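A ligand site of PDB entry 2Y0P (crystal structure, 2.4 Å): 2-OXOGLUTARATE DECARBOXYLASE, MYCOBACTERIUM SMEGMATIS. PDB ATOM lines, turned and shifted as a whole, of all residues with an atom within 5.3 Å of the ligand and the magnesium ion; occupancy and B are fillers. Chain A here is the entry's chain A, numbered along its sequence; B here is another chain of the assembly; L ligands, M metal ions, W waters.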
ATOM      1  N   PHE A 147       5.259  10.737  14.407  1.00  0.00           N
ATOM      2  CA  PHE A 147       6.259  10.249  13.428  1.00  0.00           C
ATOM      3  C   PHE A 147       7.464   9.636  14.133  1.00  0.00           C
ATOM      4  O   PHE A 147       8.555  10.204  14.125  1.00  0.00           O
ATOM      5  CB  PHE A 147       6.683  11.343  12.441  1.00  0.00           C
ATOM      6  CG  PHE A 147       5.559  11.760  11.536  1.00  0.00           C
ATOM      7  CD1 PHE A 147       5.051  10.890  10.573  1.00  0.00           C
ATOM      8  CD2 PHE A 147       4.977  13.020  11.662  1.00  0.00           C
ATOM      9  CE1 PHE A 147       4.001  11.283   9.746  1.00  0.00           C
ATOM     10  CE2 PHE A 147       3.933  13.413  10.821  1.00  0.00           C
ATOM     11  CZ  PHE A 147       3.453  12.540   9.870  1.00  0.00           C
ATOM     12  N   HIS A 180      10.390  15.209   9.800  1.00  0.00           N
ATOM     13  CA  HIS A 180       9.460  14.743  10.819  1.00  0.00           C
ATOM     14  C   HIS A 180       9.954  13.520  11.628  1.00  0.00           C
ATOM     15  O   HIS A 180       9.674  13.437  12.814  1.00  0.00           O
ATOM     16  CB  HIS A 180       8.111  14.396  10.144  1.00  0.00           C
ATOM     17  CG  HIS A 180       8.244  13.427   8.995  1.00  0.00           C
ATOM     18  ND1 HIS A 180       8.800  13.809   7.778  1.00  0.00           N
ATOM     19  CD2 HIS A 180       7.907  12.120   8.921  1.00  0.00           C
ATOM     20  CE1 HIS A 180       8.793  12.718   7.018  1.00  0.00           C
ATOM     21  NE2 HIS A 180       8.254  11.685   7.666  1.00  0.00           N
ATOM     22  N   ARG A 181      10.662  12.572  10.966  1.00  0.00           N
ATOM     23  CA  ARG A 181      11.120  11.301  11.531  1.00  0.00           C
ATOM     24  C   ARG A 181      12.039  11.489  12.760  1.00  0.00           C
ATOM     25  O   ARG A 181      13.187  11.912  12.626  1.00  0.00           O
ATOM     26  CB  ARG A 181      11.823  10.455  10.461  1.00  0.00           C
ATOM     27  CG  ARG A 181      11.982   8.959  10.793  1.00  0.00           C
ATOM     28  CD  ARG A 181      10.686   8.242  11.125  1.00  0.00           C
ATOM     29  NE  ARG A 181       9.725   8.283  10.012  1.00  0.00           N
ATOM     30  CZ  ARG A 181       8.428   8.019  10.128  1.00  0.00           C
ATOM     31  NH1 ARG A 181       7.914   7.705  11.314  1.00  0.00           N
ATOM     32  NH2 ARG A 181       7.630   8.078   9.073  1.00  0.00           N
ATOM     33  N   VAL A 217       2.531  22.684  13.696  1.00  0.00           N
ATOM     34  CA  VAL A 217       2.556  21.365  14.322  1.00  0.00           C
ATOM     35  C   VAL A 217       3.900  21.157  15.068  1.00  0.00           C
ATOM     36  O   VAL A 217       4.932  21.732  14.677  1.00  0.00           O
ATOM     37  CB  VAL A 217       2.248  20.226  13.302  1.00  0.00           C
ATOM     38  CG1 VAL A 217       0.819  20.333  12.760  1.00  0.00           C
ATOM     39  CG2 VAL A 217       3.249  20.211  12.161  1.00  0.00           C
ATOM     40  N   TYR A 219       6.097  18.721  15.338  1.00  0.00           N
ATOM     41  CA  TYR A 219       7.228  18.135  14.621  1.00  0.00           C
ATOM     42  C   TYR A 219       7.790  19.076  13.494  1.00  0.00           C
ATOM     43  O   TYR A 219       8.445  18.601  12.565  1.00  0.00           O
ATOM     44  CB  TYR A 219       6.882  16.719  14.064  1.00  0.00           C
ATOM     45  CG  TYR A 219       5.544  16.641  13.357  1.00  0.00           C
ATOM     46  CD1 TYR A 219       5.418  16.984  12.014  1.00  0.00           C
ATOM     47  CD2 TYR A 219       4.400  16.227  14.036  1.00  0.00           C
ATOM     48  CE1 TYR A 219       4.188  16.923  11.366  1.00  0.00           C
ATOM     49  CE2 TYR A 219       3.158  16.160  13.390  1.00  0.00           C
ATOM     50  CZ  TYR A 219       3.063  16.528  12.060  1.00  0.00           C
ATOM     51  OH  TYR A 219       1.847  16.465  11.402  1.00  0.00           O
ATOM     52  N   HIS A 220       7.576  20.397  13.617  1.00  0.00           N
ATOM     53  CA  HIS A 220       8.082  21.431  12.703  1.00  0.00           C
ATOM     54  C   HIS A 220       8.849  22.492  13.461  1.00  0.00           C
ATOM     55  O   HIS A 220       9.459  23.373  12.861  1.00  0.00           O
ATOM     56  CB  HIS A 220       6.920  22.125  11.968  1.00  0.00           C
ATOM     57  CG  HIS A 220       6.337  21.345  10.843  1.00  0.00           C
ATOM     58  ND1 HIS A 220       5.393  21.905  10.017  1.00  0.00           N
ATOM     59  CD2 HIS A 220       6.575  20.070  10.439  1.00  0.00           C
ATOM     60  CE1 HIS A 220       5.079  20.962   9.143  1.00  0.00           C
ATOM     61  NE2 HIS A 220       5.766  19.846   9.355  1.00  0.00           N
ATOM     62  N   PRO A 244       8.702  23.790   7.184  1.00  0.00           N
ATOM     63  CA  PRO A 244       7.347  23.364   6.844  1.00  0.00           C
ATOM     64  C   PRO A 244       7.282  21.841   6.604  1.00  0.00           C
ATOM     65  O   PRO A 244       8.273  21.134   6.825  1.00  0.00           O
ATOM     66  CB  PRO A 244       7.047  24.172   5.581  1.00  0.00           C
ATOM     67  CG  PRO A 244       8.380  24.303   4.917  1.00  0.00           C
ATOM     68  CD  PRO A 244       9.435  24.224   5.978  1.00  0.00           C
ATOM     69  N   SER A 245       6.125  21.341   6.132  1.00  0.00           N
ATOM     70  CA  SER A 245       5.939  19.924   5.817  1.00  0.00           C
ATOM     71  C   SER A 245       6.748  19.553   4.597  1.00  0.00           C
ATOM     72  O   SER A 245       7.240  18.436   4.515  1.00  0.00           O
ATOM     73  CB  SER A 245       4.471  19.586   5.589  1.00  0.00           C
ATOM     74  OG  SER A 245       3.738  19.515   6.796  1.00  0.00           O
ATOM     75  N   HIS A 246       6.907  20.525   3.664  1.00  0.00           N
ATOM     76  CA  HIS A 246       7.644  20.427   2.401  1.00  0.00           C
ATOM     77  C   HIS A 246       9.023  19.884   2.679  1.00  0.00           C
ATOM     78  O   HIS A 246       9.922  20.559   3.217  1.00  0.00           O
ATOM     79  CB  HIS A 246       7.690  21.797   1.696  1.00  0.00           C
ATOM     80  CG  HIS A 246       6.340  22.283   1.279  1.00  0.00           C
ATOM     81  ND1 HIS A 246       5.316  22.476   2.208  1.00  0.00           N
ATOM     82  CD2 HIS A 246       5.872  22.595   0.049  1.00  0.00           C
ATOM     83  CE1 HIS A 246       4.268  22.873   1.511  1.00  0.00           C
ATOM     84  NE2 HIS A 246       4.554  22.979   0.212  1.00  0.00           N
ATOM     85  N   LEU A 247       9.146  18.597   2.389  1.00  0.00           N
ATOM     86  CA  LEU A 247      10.342  17.833   2.627  1.00  0.00           C
ATOM     87  C   LEU A 247      11.495  18.376   1.827  1.00  0.00           C
ATOM     88  O   LEU A 247      11.334  18.698   0.646  1.00  0.00           O
ATOM     89  CB  LEU A 247      10.103  16.343   2.315  1.00  0.00           C
ATOM     90  CG  LEU A 247       9.155  15.617   3.278  1.00  0.00           C
ATOM     91  CD1 LEU A 247       8.795  14.252   2.769  1.00  0.00           C
ATOM     92  CD2 LEU A 247       9.766  15.514   4.670  1.00  0.00           C
ATOM     93  N   GLY A 285      15.047  11.950   4.903  1.00  0.00           N
ATOM     94  CA  GLY A 285      14.355  10.683   4.699  1.00  0.00           C
ATOM     95  C   GLY A 285      14.829  10.130   3.368  1.00  0.00           C
ATOM     96  O   GLY A 285      15.253  10.902   2.502  1.00  0.00           O
ATOM     97  N   ASP A 286      14.781   8.802   3.192  1.00  0.00           N
ATOM     98  CA  ASP A 286      15.284   8.151   1.974  1.00  0.00           C
ATOM     99  C   ASP A 286      14.489   8.499   0.701  1.00  0.00           C
ATOM    100  O   ASP A 286      15.095   8.616  -0.367  1.00  0.00           O
ATOM    101  CB  ASP A 286      15.353   6.625   2.148  1.00  0.00           C
ATOM    102  CG  ASP A 286      14.040   5.965   2.563  1.00  0.00           C
ATOM    103  OD1 ASP A 286      13.466   6.379   3.596  1.00  0.00           O
ATOM    104  OD2 ASP A 286      13.622   5.008   1.884  1.00  0.00           O
ATOM    105  N   ALA A 287      13.155   8.624   0.779  1.00  0.00           N
ATOM    106  CA  ALA A 287      12.355   8.935  -0.411  1.00  0.00           C
ATOM    107  C   ALA A 287      12.488  10.409  -0.799  1.00  0.00           C
ATOM    108  O   ALA A 287      12.559  10.721  -1.992  1.00  0.00           O
ATOM    109  CB  ALA A 287      10.890   8.572  -0.179  1.00  0.00           C
ATOM    110  N   ALA A 288      12.547  11.311   0.208  1.00  0.00           N
ATOM    111  CA  ALA A 288      12.660  12.734  -0.012  1.00  0.00           C
ATOM    112  C   ALA A 288      14.035  13.121  -0.549  1.00  0.00           C
ATOM    113  O   ALA A 288      14.116  14.006  -1.397  1.00  0.00           O
ATOM    114  CB  ALA A 288      12.358  13.476   1.271  1.00  0.00           C
ATOM    115  N   PHE A 289      15.115  12.448  -0.085  1.00  0.00           N
ATOM    116  CA  PHE A 289      16.492  12.740  -0.520  1.00  0.00           C
ATOM    117  C   PHE A 289      16.690  12.440  -2.008  1.00  0.00           C
ATOM    118  O   PHE A 289      17.336  13.220  -2.699  1.00  0.00           O
ATOM    119  CB  PHE A 289      17.516  11.958   0.313  1.00  0.00           C
ATOM    120  CG  PHE A 289      18.925  12.508   0.267  1.00  0.00           C
ATOM    121  CD1 PHE A 289      19.225  13.736   0.832  1.00  0.00           C
ATOM    122  CD2 PHE A 289      19.951  11.780  -0.314  1.00  0.00           C
ATOM    123  CE1 PHE A 289      20.543  14.230   0.834  1.00  0.00           C
ATOM    124  CE2 PHE A 289      21.259  12.283  -0.339  1.00  0.00           C
ATOM    125  CZ  PHE A 289      21.543  13.498   0.235  1.00  0.00           C
ATOM    126  N   GLN A 292      13.417  14.919  -4.171  1.00  0.00           N
ATOM    127  CA  GLN A 292      13.334  16.386  -4.166  1.00  0.00           C
ATOM    128  C   GLN A 292      14.535  17.035  -4.841  1.00  0.00           C
ATOM    129  O   GLN A 292      15.681  16.792  -4.443  1.00  0.00           O
ATOM    130  CB  GLN A 292      13.154  16.912  -2.737  1.00  0.00           C
ATOM    131  CG  GLN A 292      11.762  16.633  -2.156  1.00  0.00           C
ATOM    132  CD  GLN A 292      10.690  17.466  -2.833  1.00  0.00           C
ATOM    133  OE1 GLN A 292      10.720  18.700  -2.800  1.00  0.00           O
ATOM    134  NE2 GLN A 292       9.749  16.798  -3.481  1.00  0.00           N
ATOM    135  N   VAL A 317      18.012   8.979   7.279  1.00  0.00           N
ATOM    136  CA  VAL A 317      17.278   7.986   8.069  1.00  0.00           C
ATOM    137  C   VAL A 317      16.588   7.130   7.024  1.00  0.00           C
ATOM    138  O   VAL A 317      15.452   7.416   6.613  1.00  0.00           O
ATOM    139  CB  VAL A 317      16.321   8.618   9.116  1.00  0.00           C
ATOM    140  CG1 VAL A 317      15.612   7.542   9.955  1.00  0.00           C
ATOM    141  CG2 VAL A 317      17.052   9.615  10.022  1.00  0.00           C
ATOM    142  N   ASN A 319      14.842   4.218   6.199  1.00  0.00           N
ATOM    143  CA  ASN A 319      13.973   3.160   6.720  1.00  0.00           C
ATOM    144  C   ASN A 319      13.380   2.324   5.577  1.00  0.00           C
ATOM    145  O   ASN A 319      12.448   1.542   5.799  1.00  0.00           O
ATOM    146  CB  ASN A 319      12.866   3.732   7.638  1.00  0.00           C
ATOM    147  CG  ASN A 319      12.103   4.920   7.103  1.00  0.00           C
ATOM    148  OD1 ASN A 319      12.029   5.162   5.898  1.00  0.00           O
ATOM    149  ND2 ASN A 319      11.503   5.674   8.004  1.00  0.00           N
ATOM    150  N   GLN A 320      13.957   2.440   4.367  1.00  0.00           N
ATOM    151  CA  GLN A 320      13.645   1.683   3.146  1.00  0.00           C
ATOM    152  C   GLN A 320      12.153   1.743   2.770  1.00  0.00           C
ATOM    153  O   GLN A 320      11.614   0.781   2.225  1.00  0.00           O
ATOM    154  CB  GLN A 320      14.117   0.221   3.308  1.00  0.00           C
ATOM    155  CG  GLN A 320      15.618   0.121   3.596  1.00  0.00           C
ATOM    156  CD  GLN A 320      16.028  -1.262   3.983  1.00  0.00           C
ATOM    157  OE1 GLN A 320      16.112  -2.169   3.157  1.00  0.00           O
ATOM    158  NE2 GLN A 320      16.306  -1.448   5.263  1.00  0.00           N
ATOM    159  N   ILE A 321      11.513   2.899   3.035  1.00  0.00           N
ATOM    160  CA  ILE A 321      10.090   3.141   2.783  1.00  0.00           C
ATOM    161  C   ILE A 321       9.805   4.658   2.735  1.00  0.00           C
ATOM    162  O   ILE A 321      10.494   5.431   3.391  1.00  0.00           O
ATOM    163  CB  ILE A 321       9.214   2.404   3.884  1.00  0.00           C
ATOM    164  CG1 ILE A 321       7.720   2.329   3.502  1.00  0.00           C
ATOM    165  CG2 ILE A 321       9.406   2.948   5.312  1.00  0.00           C
ATOM    166  CD1 ILE A 321       7.396   1.319   2.503  1.00  0.00           C
ATOM    167  N   GLY A 322       8.795   5.024   1.962  1.00  0.00           N
ATOM    168  CA  GLY A 322       8.266   6.385   1.832  1.00  0.00           C
ATOM    169  C   GLY A 322       6.759   6.271   1.920  1.00  0.00           C
ATOM    170  O   GLY A 322       6.102   6.072   0.898  1.00  0.00           O
ATOM    171  N   PHE A 323       6.211   6.308   3.155  1.00  0.00           N
ATOM    172  CA  PHE A 323       4.785   6.124   3.476  1.00  0.00           C
ATOM    173  C   PHE A 323       4.361   4.686   2.995  1.00  0.00           C
ATOM    174  O   PHE A 323       4.685   3.726   3.682  1.00  0.00           O
ATOM    175  CB  PHE A 323       3.902   7.261   2.900  1.00  0.00           C
ATOM    176  CG  PHE A 323       2.505   7.467   3.470  1.00  0.00           C
ATOM    177  CD1 PHE A 323       1.863   6.438   4.160  1.00  0.00           C
ATOM    178  CD2 PHE A 323       1.811   8.641   3.238  1.00  0.00           C
ATOM    179  CE1 PHE A 323       0.583   6.625   4.679  1.00  0.00           C
ATOM    180  CE2 PHE A 323       0.516   8.816   3.736  1.00  0.00           C
ATOM    181  CZ  PHE A 323      -0.091   7.811   4.455  1.00  0.00           C
ATOM    182  N   ARG A 384      11.147   1.225   9.790  1.00  0.00           N
ATOM    183  CA  ARG A 384      10.090   1.990  10.457  1.00  0.00           C
ATOM    184  C   ARG A 384       9.187   0.960  11.147  1.00  0.00           C
ATOM    185  O   ARG A 384       8.458   0.248  10.473  1.00  0.00           O
ATOM    186  CB  ARG A 384       9.360   2.845   9.407  1.00  0.00           C
ATOM    187  CG  ARG A 384       8.392   3.880   9.960  1.00  0.00           C
ATOM    188  CD  ARG A 384       7.429   4.298   8.876  1.00  0.00           C
ATOM    189  NE  ARG A 384       6.610   3.164   8.434  1.00  0.00           N
ATOM    190  CZ  ARG A 384       6.015   3.084   7.244  1.00  0.00           C
ATOM    191  NH1 ARG A 384       6.141   4.065   6.366  1.00  0.00           N
ATOM    192  NH2 ARG A 384       5.306   2.007   6.922  1.00  0.00           N
ATOM    193  N   HIS A 388       3.484   4.656   8.651  1.00  0.00           N
ATOM    194  CA  HIS A 388       4.058   5.961   8.333  1.00  0.00           C
ATOM    195  C   HIS A 388       3.852   6.923   9.498  1.00  0.00           C
ATOM    196  O   HIS A 388       4.809   7.544   9.961  1.00  0.00           O
ATOM    197  CB  HIS A 388       3.434   6.497   7.042  1.00  0.00           C
ATOM    198  CG  HIS A 388       3.914   7.843   6.623  1.00  0.00           C
ATOM    199  ND1 HIS A 388       5.239   8.052   6.290  1.00  0.00           N
ATOM    200  CD2 HIS A 388       3.226   8.994   6.448  1.00  0.00           C
ATOM    201  CE1 HIS A 388       5.321   9.332   5.946  1.00  0.00           C
ATOM    202  NE2 HIS A 388       4.131   9.932   6.020  1.00  0.00           N
ATOM    203  N   GLN B 542       1.698  10.580  -5.133  1.00  0.00           N
ATOM    204  CA  GLN B 542       2.319  10.025  -3.942  1.00  0.00           C
ATOM    205  C   GLN B 542       1.323   9.145  -3.171  1.00  0.00           C
ATOM    206  O   GLN B 542       0.295   9.641  -2.700  1.00  0.00           O
ATOM    207  CB  GLN B 542       2.900  11.145  -3.062  1.00  0.00           C
ATOM    208  CG  GLN B 542       4.245  11.662  -3.568  1.00  0.00           C
ATOM    209  CD  GLN B 542       4.492  13.116  -3.260  1.00  0.00           C
ATOM    210  OE1 GLN B 542       3.963  13.676  -2.295  1.00  0.00           O
ATOM    211  NE2 GLN B 542       5.342  13.749  -4.063  1.00  0.00           N
ATOM    212  N   ASP B 543       1.610   7.819  -3.103  1.00  0.00           N
ATOM    213  CA  ASP B 543       0.820   6.798  -2.420  1.00  0.00           C
ATOM    214  C   ASP B 543      -0.611   6.700  -3.012  1.00  0.00           C
ATOM    215  O   ASP B 543      -1.551   6.356  -2.305  1.00  0.00           O
ATOM    216  CB  ASP B 543       0.782   7.095  -0.898  1.00  0.00           C
ATOM    217  CG  ASP B 543       2.172   7.297  -0.309  1.00  0.00           C
ATOM    218  OD1 ASP B 543       2.912   6.299  -0.192  1.00  0.00           O
ATOM    219  OD2 ASP B 543       2.510   8.456   0.012  1.00  0.00           O
ATOM    220  N   LEU B 591       8.947  10.958  -4.722  1.00  0.00           N
ATOM    221  CA  LEU B 591       8.596  12.070  -3.850  1.00  0.00           C
ATOM    222  C   LEU B 591       9.010  13.379  -4.516  1.00  0.00           C
ATOM    223  O   LEU B 591       9.903  14.085  -4.058  1.00  0.00           O
ATOM    224  CB  LEU B 591       9.195  11.932  -2.439  1.00  0.00           C
ATOM    225  CG  LEU B 591       8.266  12.374  -1.301  1.00  0.00           C
ATOM    226  CD1 LEU B 591       8.683  11.738  -0.009  1.00  0.00           C
ATOM    227  CD2 LEU B 591       8.200  13.893  -1.167  1.00  0.00           C
ATOM    228  N   GLU B 593       7.153  16.791  -7.028  1.00  0.00           N
ATOM    229  CA  GLU B 593       5.962  17.516  -7.447  1.00  0.00           C
ATOM    230  C   GLU B 593       6.276  18.119  -8.805  1.00  0.00           C
ATOM    231  O   GLU B 593       5.549  17.826  -9.762  1.00  0.00           O
ATOM    232  CB  GLU B 593       5.550  18.574  -6.414  1.00  0.00           C
ATOM    233  CG  GLU B 593       4.889  17.997  -5.183  1.00  0.00           C
ATOM    234  CD  GLU B 593       5.789  17.443  -4.092  1.00  0.00           C
ATOM    235  OE1 GLU B 593       6.979  17.835  -4.018  1.00  0.00           O
ATOM    236  OE2 GLU B 593       5.288  16.624  -3.287  1.00  0.00           O
ATOM    237  N   GLN B 617      -0.410  14.591  -2.539  1.00  0.00           N
ATOM    238  CA  GLN B 617      -0.625  13.951  -1.246  1.00  0.00           C
ATOM    239  C   GLN B 617      -1.644  14.809  -0.489  1.00  0.00           C
ATOM    240  O   GLN B 617      -2.664  14.301  -0.002  1.00  0.00           O
ATOM    241  CB  GLN B 617       0.692  13.794  -0.474  1.00  0.00           C
ATOM    242  CG  GLN B 617       0.575  12.959   0.817  1.00  0.00           C
ATOM    243  CD  GLN B 617       1.219  11.607   0.673  1.00  0.00           C
ATOM    244  OE1 GLN B 617       2.350  11.378   1.110  1.00  0.00           O
ATOM    245  NE2 GLN B 617       0.530  10.684   0.027  1.00  0.00           N
ATOM    246  N   PHE B 618      -1.371  16.131  -0.465  1.00  0.00           N
ATOM    247  CA  PHE B 618      -2.162  17.248   0.052  1.00  0.00           C
ATOM    248  C   PHE B 618      -1.951  18.372  -0.939  1.00  0.00           C
ATOM    249  O   PHE B 618      -0.841  18.502  -1.458  1.00  0.00           O
ATOM    250  CB  PHE B 618      -1.726  17.639   1.476  1.00  0.00           C
ATOM    251  CG  PHE B 618      -2.136  16.682   2.574  1.00  0.00           C
ATOM    252  CD1 PHE B 618      -1.360  15.563   2.861  1.00  0.00           C
ATOM    253  CD2 PHE B 618      -3.272  16.906   3.334  1.00  0.00           C
ATOM    254  CE1 PHE B 618      -1.738  14.669   3.871  1.00  0.00           C
ATOM    255  CE2 PHE B 618      -3.640  16.032   4.355  1.00  0.00           C
ATOM    256  CZ  PHE B 618      -2.863  14.913   4.612  1.00  0.00           C
ATOM    257  N   PHE B 621       1.196  20.852  -1.366  1.00  0.00           N
ATOM    258  CA  PHE B 621       2.495  20.537  -1.966  1.00  0.00           C
ATOM    259  C   PHE B 621       2.570  20.862  -3.455  1.00  0.00           C
ATOM    260  O   PHE B 621       3.668  20.788  -4.028  1.00  0.00           O
ATOM    261  CB  PHE B 621       2.837  19.045  -1.734  1.00  0.00           C
ATOM    262  CG  PHE B 621       2.835  18.670  -0.275  1.00  0.00           C
ATOM    263  CD1 PHE B 621       3.682  19.328   0.624  1.00  0.00           C
ATOM    264  CD2 PHE B 621       1.935  17.736   0.223  1.00  0.00           C
ATOM    265  CE1 PHE B 621       3.639  19.017   1.988  1.00  0.00           C
ATOM    266  CE2 PHE B 621       1.906  17.424   1.578  1.00  0.00           C
ATOM    267  CZ  PHE B 621       2.751  18.076   2.454  1.00  0.00           C
ATOM    268  N   HIS B 661      -1.368  21.012   5.613  1.00  0.00           N
ATOM    269  CA  HIS B 661      -2.309  19.914   5.426  1.00  0.00           C
ATOM    270  C   HIS B 661      -3.731  20.483   5.420  1.00  0.00           C
ATOM    271  O   HIS B 661      -4.648  19.885   5.973  1.00  0.00           O
ATOM    272  CB  HIS B 661      -2.113  18.851   6.529  1.00  0.00           C
ATOM    273  CG  HIS B 661      -0.785  18.164   6.468  1.00  0.00           C
ATOM    274  ND1 HIS B 661      -0.610  17.003   5.745  1.00  0.00           N
ATOM    275  CD2 HIS B 661       0.404  18.524   7.009  1.00  0.00           C
ATOM    276  CE1 HIS B 661       0.663  16.681   5.891  1.00  0.00           C
ATOM    277  NE2 HIS B 661       1.311  17.577   6.628  1.00  0.00           N
HETATM  278  O1  LIG L   1       8.480   9.077   6.550  1.00  0.00           O
HETATM  279  P1  LIG L   1      10.017   8.751   6.239  1.00  0.00           P
HETATM  280  O2  LIG L   1      10.158   7.323   5.868  1.00  0.00           O
HETATM  281  O3  LIG L   1      10.946   9.044   7.524  1.00  0.00           O
HETATM  282  O4  LIG L   1      10.501   9.665   5.135  1.00  0.00           O
HETATM  283  P2  LIG L   1      10.650   9.593   3.539  1.00  0.00           P
HETATM  284  O5  LIG L   1      11.481  10.733   3.054  1.00  0.00           O
HETATM  285  O6  LIG L   1      11.340   8.199   3.139  1.00  0.00           O
HETATM  286  O7  LIG L   1       9.185   9.714   2.852  1.00  0.00           O
HETATM  287  C1  LIG L   1       8.096  10.354   3.509  1.00  0.00           C
HETATM  288  C2  LIG L   1       6.833  10.436   2.638  1.00  0.00           C
HETATM  289  C3  LIG L   1       6.079  11.680   3.045  1.00  0.00           C
HETATM  290  S1  LIG L   1       6.064  12.319   4.685  1.00  0.00           S
HETATM  291  C4  LIG L   1       5.382  12.539   2.284  1.00  0.00           C
HETATM  292  C5  LIG L   1       5.265  12.229   0.820  1.00  0.00           C
HETATM  293  N1  LIG L   1       4.842  13.570   2.905  1.00  0.00           N
HETATM  294  C6  LIG L   1       5.058  13.603   4.185  1.00  0.00           C
HETATM  295  O8  LIG L   1       3.247  15.175   5.085  1.00  0.00           O
HETATM  296  C7  LIG L   1       5.432  14.929   6.368  1.00  0.00           C
HETATM  297  C8  LIG L   1       4.611  16.601   7.954  1.00  0.00           C
HETATM  298  O9  LIG L   1       3.513  17.177   8.035  1.00  0.00           O
HETATM  299  O10 LIG L   1       5.699  17.200   8.120  1.00  0.00           O
HETATM  300  C9  LIG L   1       4.029  14.589   2.207  1.00  0.00           C
HETATM  301  C10 LIG L   1       4.913  15.524   1.404  1.00  0.00           C
HETATM  302  C11 LIG L   1       4.872  15.497   0.020  1.00  0.00           C
HETATM  303  N2  LIG L   1       5.659  16.326  -0.683  1.00  0.00           N
HETATM  304  C12 LIG L   1       6.470  17.179  -0.063  1.00  0.00           C
HETATM  305  C13 LIG L   1       7.334  18.102  -0.874  1.00  0.00           C
HETATM  306  N3  LIG L   1       6.531  17.256   1.260  1.00  0.00           N
HETATM  307  C14 LIG L   1       5.788  16.442   2.019  1.00  0.00           C
HETATM  308  C15 LIG L   1       4.623  15.120   7.645  1.00  0.00           C
HETATM  309  N4  LIG L   1       5.867  16.573   3.394  1.00  0.00           N
HETATM  310  C16 LIG L   1       4.534  14.588   5.204  1.00  0.00           C
HETATM  311 MG    MG M   1      11.629   6.566   4.491  1.00  0.00          MG
HETATM  312  O   HOH W   1       7.386   6.357   5.515  1.00  0.00           O
HETATM  313  O   HOH W   2      13.042   7.798   5.970  1.00  0.00           O
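The side-chain hydroxyl (OG) of Ser 245 sits at hydrogen-bond distance from a ring nitrogen (NE2) of His 661 of chain B, 3.1 Å away.
OG of Ser 245 lies close to NE2 of His 220, at 3.3 Å.
The side-chain amide nitrogen (NE2) of Gln 542 of chain B sits at hydrogen-bond distance from the side-chain carboxylate (OE2) of Glu 593 of chain B.
The side-chain amide nitrogen (NE2) of Gln 292 sits at hydrogen-bond distance from the side-chain carboxylate (OE1) of Glu 593 of chain B, at 3.0 Å.
NH2 of Arg 181 sits at hydrogen-bond distance from O of His 388 (3.0 Å).
O of Gln 542 of chain B lies within hydrogen-bond range of NE2 of Gln 617 of chain B (2.9 Å).
The side-chain amide nitrogen of Gln 617 of chain B lies within hydrogen-bond range of the side-chain carboxylate of Asp 543 of chain B, at 3.0 Å.
O of Leu 591 of chain B sits at hydrogen-bond distance from NE2 of Gln 292 (2.8 Å).
The magnesium ion is bound by the backbone carbonyl oxygen (O) of Ile 321 (1.9 Å), the side-chain amide oxygen (OD1) of Asn 319 (2.0 Å), the side-chain carboxylate (OD1) of Asp 286 (2.1 Å), an oxygen (O6) of the ligand (2.1 Å), an oxygen (O2) of the ligand (2.2 Å) and water W2 (2.4 Å).
O6 of the ligand sits close to N of Asp 286 (3.5 Å).
The backbone carbonyl oxygen of Ser 245 sits at hydrogen-bond distance from a nitrogen (N4) of the ligand (2.6 Å).
The side-chain hydroxyl of Ser 245 sits at hydrogen-bond distance from an oxygen (O9) of the ligand, 2.7 Å away.
A ring nitrogen (NE2) of His 661 of chain B lies within hydrogen-bond range of an oxygen (O9) of the ligand (2.6 Å).
The side-chain carboxylate of Glu 593 of chain B lies within hydrogen-bond range of a nitrogen (N2) of the ligand (2.6 Å).
The guanidinium group of Arg 181 is in salt-bridge range of an oxygen (O1) of the ligand.
NE2 of His 180 lies within hydrogen-bond range of O1 of the ligand.
An oxygen (O10) of the ligand lies within hydrogen-bond range of a ring nitrogen (NE2) of His 220 (2.9 Å).
O6 of the ligand lies close to N of Ala 287 (3.0 Å).
N of Ala 288 lies within hydrogen-bond range of O5 of the ligand.
The backbone NH (N) of Leu 247 sits at hydrogen-bond distance from a nitrogen (N3) of the ligand, at 3.1 Å.
S1 of the ligand sits close to NE2 of His 388, 3.3 Å away.
Water W2 lies within hydrogen-bond range of O of Val 317 (2.5 Å), O3 of the ligand (2.9 Å), ND2 of Asn 319 (3.3 Å) and N of Asp 286 (3.4 Å).
Water W1 lies within hydrogen-bond range of N of Phe 323 (2.6 Å), NH1 of Arg 384 (2.7 Å), ND1 of His 388 (2.8 Å) and O1 of the ligand (3.1 Å).
Phe 147 touches the ligand (CZ to C15, 3.6 Å).
Tyr 219 touches the ligand.
His 246 touches the ligand (CA to N3, 3.5 Å).
Gly 285 touches the ligand.
Gln 292 touches the ligand.
Gly 322 touches the ligand (CA to O7, 3.6 Å).
Gln 542 of chain B touches the ligand (OE1 to C11, 3.1 Å).
CD1 of Leu 591 of chain B touches C2 of the ligand, at 3.5 Å.
Gln 617 of chain B touches the ligand.
Phe 621 of chain B touches the ligand (CE1 to C14, 3.4 Å).
Hydrophobic or aromatic side chains that line the ligand: Phe 147, His 180, Tyr 219, His 220, Leu 247, Ala 287, Ala 288, His 388, Leu 591 of chain B, Phe 621 of chain B and His 661 of chain B.
The nearest printed residue that does not touch the ligand is Phe 323 (4.2 Å).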
